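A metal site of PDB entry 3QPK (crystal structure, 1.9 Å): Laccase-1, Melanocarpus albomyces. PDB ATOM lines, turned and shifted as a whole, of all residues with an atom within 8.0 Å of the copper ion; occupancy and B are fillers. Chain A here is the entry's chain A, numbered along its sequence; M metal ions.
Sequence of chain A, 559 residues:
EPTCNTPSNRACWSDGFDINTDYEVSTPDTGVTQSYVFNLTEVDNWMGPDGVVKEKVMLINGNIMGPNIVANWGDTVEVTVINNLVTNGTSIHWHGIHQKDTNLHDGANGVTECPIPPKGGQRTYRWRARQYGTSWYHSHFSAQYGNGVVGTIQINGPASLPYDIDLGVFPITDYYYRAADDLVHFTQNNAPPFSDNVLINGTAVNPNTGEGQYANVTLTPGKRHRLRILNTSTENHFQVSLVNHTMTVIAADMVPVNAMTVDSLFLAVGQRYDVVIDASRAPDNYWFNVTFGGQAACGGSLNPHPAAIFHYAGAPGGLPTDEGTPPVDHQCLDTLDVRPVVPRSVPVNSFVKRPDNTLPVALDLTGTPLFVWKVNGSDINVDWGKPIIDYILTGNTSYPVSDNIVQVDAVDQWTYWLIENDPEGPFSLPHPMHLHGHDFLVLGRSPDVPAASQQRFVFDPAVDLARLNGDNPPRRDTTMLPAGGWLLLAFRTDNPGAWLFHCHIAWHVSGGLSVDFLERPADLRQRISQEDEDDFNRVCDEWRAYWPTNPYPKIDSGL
The copper ion is bound by ND1 of His 431 (2.0 Å), SG of Cys 503 (2.1 Å) and ND1 of His 508 (2.2 Å).
A ring nitrogen (NE2) of His 431 sits close to the backbone carbonyl oxygen of Leu 429, 3.1 Å away.
The backbone carbonyl oxygen (O) of His 431 is in hydrogen-bond range of the backbone NH (N) of Leu 481.
N of Ile 505 sits close to SG of Cys 503.
N of Cys 503 is in hydrogen-bond range of O of Leu 513 (3.3 Å).
The backbone NH (N) of Leu 513 is in hydrogen-bond range of the backbone carbonyl oxygen (O) of His 508 (3.0 Å).
Ile 505 touches the copper ion (CD1 to CU, 3.8 Å).
Leu 513 touches the copper ion (CD1 to CU, 3.8 Å).
Five residues have an atom within 4 Å of the copper ion: His 431, Cys 503, Ile 505, His 508 and Leu 513.
The nearest printed residue that does not touch the copper ion is Pro 432 (4.3 Å).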
ATOM      1  N   GLU A 235      31.488  19.035  11.386  1.00  0.00           N
ATOM      2  CA  GLU A 235      30.540  17.942  11.078  1.00  0.00           C
ATOM      3  C   GLU A 235      30.546  16.775  12.089  1.00  0.00           C
ATOM      4  O   GLU A 235      29.492  16.246  12.468  1.00  0.00           O
ATOM      5  CB  GLU A 235      30.809  17.394   9.672  1.00  0.00           C
ATOM      6  CG  GLU A 235      29.724  16.437   9.119  1.00  0.00           C
ATOM      7  CD  GLU A 235      29.910  14.995   9.558  1.00  0.00           C
ATOM      8  OE1 GLU A 235      30.981  14.667  10.105  1.00  0.00           O
ATOM      9  OE2 GLU A 235      28.981  14.177   9.355  1.00  0.00           O
ATOM     10  N   HIS A 237      30.385  14.365  15.088  1.00  0.00           N
ATOM     11  CA  HIS A 237      29.732  14.266  16.388  1.00  0.00           C
ATOM     12  C   HIS A 237      30.444  13.185  17.194  1.00  0.00           C
ATOM     13  O   HIS A 237      30.619  12.078  16.699  1.00  0.00           O
ATOM     14  CB  HIS A 237      28.287  13.854  16.216  1.00  0.00           C
ATOM     15  CG  HIS A 237      27.419  14.849  15.512  1.00  0.00           C
ATOM     16  ND1 HIS A 237      27.701  15.318  14.245  1.00  0.00           N
ATOM     17  CD2 HIS A 237      26.233  15.404  15.858  1.00  0.00           C
ATOM     18  CE1 HIS A 237      26.756  16.155  13.868  1.00  0.00           C
ATOM     19  NE2 HIS A 237      25.843  16.213  14.826  1.00  0.00           N
ATOM     20  N   VAL A 361      11.930  20.149   8.022  1.00  0.00           N
ATOM     21  CA  VAL A 361      13.219  20.055   7.331  1.00  0.00           C
ATOM     22  C   VAL A 361      13.099  19.153   6.109  1.00  0.00           C
ATOM     23  O   VAL A 361      12.547  18.060   6.198  1.00  0.00           O
ATOM     24  CB  VAL A 361      14.301  19.515   8.282  1.00  0.00           C
ATOM     25  CG1 VAL A 361      15.604  19.330   7.564  1.00  0.00           C
ATOM     26  CG2 VAL A 361      14.475  20.498   9.480  1.00  0.00           C
ATOM     27  N   TRP A 373      19.241  22.014   1.235  1.00  0.00           N
ATOM     28  CA  TRP A 373      18.420  21.834   2.419  1.00  0.00           C
ATOM     29  C   TRP A 373      17.421  22.953   2.549  1.00  0.00           C
ATOM     30  O   TRP A 373      17.746  24.118   2.329  1.00  0.00           O
ATOM     31  CB  TRP A 373      19.300  21.788   3.661  1.00  0.00           C
ATOM     32  CG  TRP A 373      20.174  20.597   3.665  1.00  0.00           C
ATOM     33  CD1 TRP A 373      21.448  20.518   3.181  1.00  0.00           C
ATOM     34  CD2 TRP A 373      19.851  19.307   4.147  1.00  0.00           C
ATOM     35  NE1 TRP A 373      21.934  19.249   3.358  1.00  0.00           N
ATOM     36  CE2 TRP A 373      20.968  18.487   3.954  1.00  0.00           C
ATOM     37  CE3 TRP A 373      18.712  18.747   4.759  1.00  0.00           C
ATOM     38  CZ2 TRP A 373      20.987  17.137   4.322  1.00  0.00           C
ATOM     39  CZ3 TRP A 373      18.739  17.420   5.126  1.00  0.00           C
ATOM     40  CH2 TRP A 373      19.865  16.635   4.913  1.00  0.00           C
ATOM     41  N   ASN A 421      12.032  16.167  10.683  1.00  0.00           N
ATOM     42  CA  ASN A 421      13.214  15.790   9.909  1.00  0.00           C
ATOM     43  C   ASN A 421      12.918  15.008   8.627  1.00  0.00           C
ATOM     44  O   ASN A 421      13.288  13.833   8.509  1.00  0.00           O
ATOM     45  CB  ASN A 421      14.191  15.033  10.805  1.00  0.00           C
ATOM     46  CG  ASN A 421      15.586  14.982  10.222  1.00  0.00           C
ATOM     47  OD1 ASN A 421      15.824  15.474   9.115  1.00  0.00           O
ATOM     48  ND2 ASN A 421      16.513  14.380  10.948  1.00  0.00           N
ATOM     49  N   LEU A 429      18.895  12.417   7.895  1.00  0.00           N
ATOM     50  CA  LEU A 429      20.125  12.433   8.668  1.00  0.00           C
ATOM     51  C   LEU A 429      19.863  13.121   9.997  1.00  0.00           C
ATOM     52  O   LEU A 429      19.027  14.014  10.075  1.00  0.00           O
ATOM     53  CB  LEU A 429      21.178  13.231   7.905  1.00  0.00           C
ATOM     54  CG  LEU A 429      21.417  12.950   6.430  1.00  0.00           C
ATOM     55  CD1 LEU A 429      22.419  13.933   5.871  1.00  0.00           C
ATOM     56  CD2 LEU A 429      21.870  11.504   6.228  1.00  0.00           C
ATOM     57  N   PRO A 430      20.603  12.718  11.034  1.00  0.00           N
ATOM     58  CA  PRO A 430      20.631  13.462  12.295  1.00  0.00           C
ATOM     59  C   PRO A 430      21.150  14.871  12.057  1.00  0.00           C
ATOM     60  O   PRO A 430      22.101  15.055  11.275  1.00  0.00           O
ATOM     61  CB  PRO A 430      21.638  12.681  13.150  1.00  0.00           C
ATOM     62  CG  PRO A 430      21.739  11.296  12.485  1.00  0.00           C
ATOM     63  CD  PRO A 430      21.549  11.590  11.022  1.00  0.00           C
ATOM     64  N   HIS A 431      20.556  15.863  12.713  1.00  0.00           N
ATOM     65  CA  HIS A 431      21.069  17.217  12.644  1.00  0.00           C
ATOM     66  C   HIS A 431      21.227  17.831  14.044  1.00  0.00           C
ATOM     67  O   HIS A 431      20.288  17.820  14.868  1.00  0.00           O
ATOM     68  CB  HIS A 431      20.143  18.102  11.820  1.00  0.00           C
ATOM     69  CG  HIS A 431      19.878  17.592  10.433  1.00  0.00           C
ATOM     70  ND1 HIS A 431      20.695  17.876   9.369  1.00  0.00           N
ATOM     71  CD2 HIS A 431      18.855  16.857   9.932  1.00  0.00           C
ATOM     72  CE1 HIS A 431      20.206  17.334   8.274  1.00  0.00           C
ATOM     73  NE2 HIS A 431      19.090  16.697   8.586  1.00  0.00           N
ATOM     74  N   PRO A 432      22.414  18.381  14.329  1.00  0.00           N
ATOM     75  CA  PRO A 432      22.537  19.130  15.590  1.00  0.00           C
ATOM     76  C   PRO A 432      21.926  20.524  15.473  1.00  0.00           C
ATOM     77  O   PRO A 432      22.519  21.389  14.828  1.00  0.00           O
ATOM     78  CB  PRO A 432      24.050  19.233  15.801  1.00  0.00           C
ATOM     79  CG  PRO A 432      24.649  19.037  14.412  1.00  0.00           C
ATOM     80  CD  PRO A 432      23.646  18.364  13.536  1.00  0.00           C
ATOM     81  N   MET A 433      20.769  20.721  16.096  1.00  0.00           N
ATOM     82  CA  MET A 433      20.033  21.974  15.993  1.00  0.00           C
ATOM     83  C   MET A 433      20.448  22.982  17.064  1.00  0.00           C
ATOM     84  O   MET A 433      20.441  22.675  18.263  1.00  0.00           O
ATOM     85  CB  MET A 433      18.517  21.716  16.078  1.00  0.00           C
ATOM     86  CG  MET A 433      17.998  20.836  14.945  1.00  0.00           C
ATOM     87  SD  MET A 433      18.536  21.381  13.310  1.00  0.00           S
ATOM     88  CE  MET A 433      17.392  22.726  13.028  1.00  0.00           C
ATOM     89  N   MET A 480      20.056  17.172  19.470  1.00  0.00           N
ATOM     90  CA  MET A 480      19.906  16.395  18.240  1.00  0.00           C
ATOM     91  C   MET A 480      18.463  16.303  17.715  1.00  0.00           C
ATOM     92  O   MET A 480      17.512  16.071  18.479  1.00  0.00           O
ATOM     93  CB  MET A 480      20.553  15.012  18.374  1.00  0.00           C
ATOM     94  CG  MET A 480      22.076  15.066  18.625  1.00  0.00           C
ATOM     95  SD  MET A 480      22.965  15.851  17.267  1.00  0.00           S
ATOM     96  CE  MET A 480      22.478  14.694  15.930  1.00  0.00           C
ATOM     97  N   LEU A 481      18.318  16.529  16.416  1.00  0.00           N
ATOM     98  CA  LEU A 481      17.096  16.243  15.682  1.00  0.00           C
ATOM     99  C   LEU A 481      17.237  14.827  15.119  1.00  0.00           C
ATOM    100  O   LEU A 481      18.072  14.591  14.233  1.00  0.00           O
ATOM    101  CB  LEU A 481      16.914  17.254  14.561  1.00  0.00           C
ATOM    102  CG  LEU A 481      15.750  17.109  13.588  1.00  0.00           C
ATOM    103  CD1 LEU A 481      14.383  17.126  14.301  1.00  0.00           C
ATOM    104  CD2 LEU A 481      15.820  18.191  12.514  1.00  0.00           C
ATOM    105  N   HIS A 502      19.452  26.799  13.373  1.00  0.00           N
ATOM    106  CA  HIS A 502      19.988  26.048  12.251  1.00  0.00           C
ATOM    107  C   HIS A 502      20.740  24.796  12.677  1.00  0.00           C
ATOM    108  O   HIS A 502      21.095  24.639  13.838  1.00  0.00           O
ATOM    109  CB  HIS A 502      20.899  26.960  11.434  1.00  0.00           C
ATOM    110  CG  HIS A 502      22.140  27.380  12.157  1.00  0.00           C
ATOM    111  ND1 HIS A 502      23.314  26.668  12.108  1.00  0.00           N
ATOM    112  CD2 HIS A 502      22.391  28.458  12.939  1.00  0.00           C
ATOM    113  CE1 HIS A 502      24.242  27.273  12.834  1.00  0.00           C
ATOM    114  NE2 HIS A 502      23.713  28.369  13.351  1.00  0.00           N
ATOM    115  N   CYS A 503      20.938  23.888  11.717  1.00  0.00           N
ATOM    116  CA  CYS A 503      21.849  22.765  11.913  1.00  0.00           C
ATOM    117  C   CYS A 503      23.279  23.320  12.007  1.00  0.00           C
ATOM    118  O   CYS A 503      23.636  24.240  11.261  1.00  0.00           O
ATOM    119  CB  CYS A 503      21.769  21.793  10.744  1.00  0.00           C
ATOM    120  SG  CYS A 503      22.974  20.507  10.923  1.00  0.00           S
ATOM    121  N   HIS A 504      24.079  22.771  12.911  1.00  0.00           N
ATOM    122  CA  HIS A 504      25.444  23.289  13.111  1.00  0.00           C
ATOM    123  C   HIS A 504      26.523  22.567  12.300  1.00  0.00           C
ATOM    124  O   HIS A 504      27.713  22.864  12.460  1.00  0.00           O
ATOM    125  CB  HIS A 504      25.838  23.263  14.592  1.00  0.00           C
ATOM    126  CG  HIS A 504      26.812  24.346  14.970  1.00  0.00           C
ATOM    127  ND1 HIS A 504      28.129  24.338  14.576  1.00  0.00           N
ATOM    128  CD2 HIS A 504      26.643  25.473  15.702  1.00  0.00           C
ATOM    129  CE1 HIS A 504      28.731  25.414  15.049  1.00  0.00           C
ATOM    130  NE2 HIS A 504      27.844  26.121  15.728  1.00  0.00           N
ATOM    131  N   ILE A 505      26.105  21.619  11.459  1.00  0.00           N
ATOM    132  CA  ILE A 505      27.031  20.986  10.520  1.00  0.00           C
ATOM    133  C   ILE A 505      27.262  22.001   9.421  1.00  0.00           C
ATOM    134  O   ILE A 505      26.337  22.377   8.702  1.00  0.00           O
ATOM    135  CB  ILE A 505      26.430  19.697   9.934  1.00  0.00           C
ATOM    136  CG1 ILE A 505      26.331  18.611  11.017  1.00  0.00           C
ATOM    137  CG2 ILE A 505      27.275  19.191   8.757  1.00  0.00           C
ATOM    138  CD1 ILE A 505      25.572  17.379  10.550  1.00  0.00           C
ATOM    139  N   ALA A 506      28.489  22.501   9.341  1.00  0.00           N
ATOM    140  CA  ALA A 506      28.846  23.569   8.410  1.00  0.00           C
ATOM    141  C   ALA A 506      28.284  23.375   7.002  1.00  0.00           C
ATOM    142  O   ALA A 506      27.855  24.338   6.376  1.00  0.00           O
ATOM    143  CB  ALA A 506      30.377  23.734   8.361  1.00  0.00           C
ATOM    144  N   TRP A 507      28.311  22.146   6.494  1.00  0.00           N
ATOM    145  CA  TRP A 507      27.867  21.897   5.125  1.00  0.00           C
ATOM    146  C   TRP A 507      26.356  22.005   4.973  1.00  0.00           C
ATOM    147  O   TRP A 507      25.867  22.343   3.897  1.00  0.00           O
ATOM    148  CB  TRP A 507      28.362  20.538   4.620  1.00  0.00           C
ATOM    149  CG  TRP A 507      29.624  20.028   5.270  1.00  0.00           C
ATOM    150  CD1 TRP A 507      29.794  18.832   5.886  1.00  0.00           C
ATOM    151  CD2 TRP A 507      30.873  20.706   5.356  1.00  0.00           C
ATOM    152  NE1 TRP A 507      31.078  18.719   6.363  1.00  0.00           N
ATOM    153  CE2 TRP A 507      31.767  19.861   6.043  1.00  0.00           C
ATOM    154  CE3 TRP A 507      31.328  21.953   4.929  1.00  0.00           C
ATOM    155  CZ2 TRP A 507      33.083  20.213   6.309  1.00  0.00           C
ATOM    156  CZ3 TRP A 507      32.645  22.314   5.201  1.00  0.00           C
ATOM    157  CH2 TRP A 507      33.506  21.453   5.879  1.00  0.00           C
ATOM    158  N   HIS A 508      25.614  21.754   6.051  1.00  0.00           N
ATOM    159  CA  HIS A 508      24.144  21.802   5.994  1.00  0.00           C
ATOM    160  C   HIS A 508      23.556  23.223   6.137  1.00  0.00           C
ATOM    161  O   HIS A 508      22.636  23.588   5.395  1.00  0.00           O
ATOM    162  CB  HIS A 508      23.542  20.868   7.042  1.00  0.00           C
ATOM    163  CG  HIS A 508      23.875  19.424   6.832  1.00  0.00           C
ATOM    164  ND1 HIS A 508      23.551  18.447   7.743  1.00  0.00           N
ATOM    165  CD2 HIS A 508      24.503  18.792   5.809  1.00  0.00           C
ATOM    166  CE1 HIS A 508      23.977  17.278   7.300  1.00  0.00           C
ATOM    167  NE2 HIS A 508      24.542  17.463   6.119  1.00  0.00           N
ATOM    168  N   VAL A 509      24.061  23.999   7.095  1.00  0.00           N
ATOM    169  CA  VAL A 509      23.664  25.403   7.168  1.00  0.00           C
ATOM    170  C   VAL A 509      24.148  26.122   5.908  1.00  0.00           C
ATOM    171  O   VAL A 509      23.455  26.989   5.376  1.00  0.00           O
ATOM    172  CB  VAL A 509      24.110  26.128   8.487  1.00  0.00           C
ATOM    173  CG1 VAL A 509      25.610  26.265   8.585  1.00  0.00           C
ATOM    174  CG2 VAL A 509      23.403  27.504   8.641  1.00  0.00           C
ATOM    175  N   LEU A 513      20.031  25.013   5.580  1.00  0.00           N
ATOM    176  CA  LEU A 513      19.315  24.506   6.749  1.00  0.00           C
ATOM    177  C   LEU A 513      19.301  25.465   7.951  1.00  0.00           C
ATOM    178  O   LEU A 513      20.065  25.308   8.908  1.00  0.00           O
ATOM    179  CB  LEU A 513      19.870  23.140   7.175  1.00  0.00           C
ATOM    180  CG  LEU A 513      18.805  22.125   7.602  1.00  0.00           C
ATOM    181  CD1 LEU A 513      19.407  20.727   7.784  1.00  0.00           C
ATOM    182  CD2 LEU A 513      18.131  22.569   8.879  1.00  0.00           C
HETATM  183 CU    CU M   1      22.353  19.039   9.535  1.00  0.00          CU
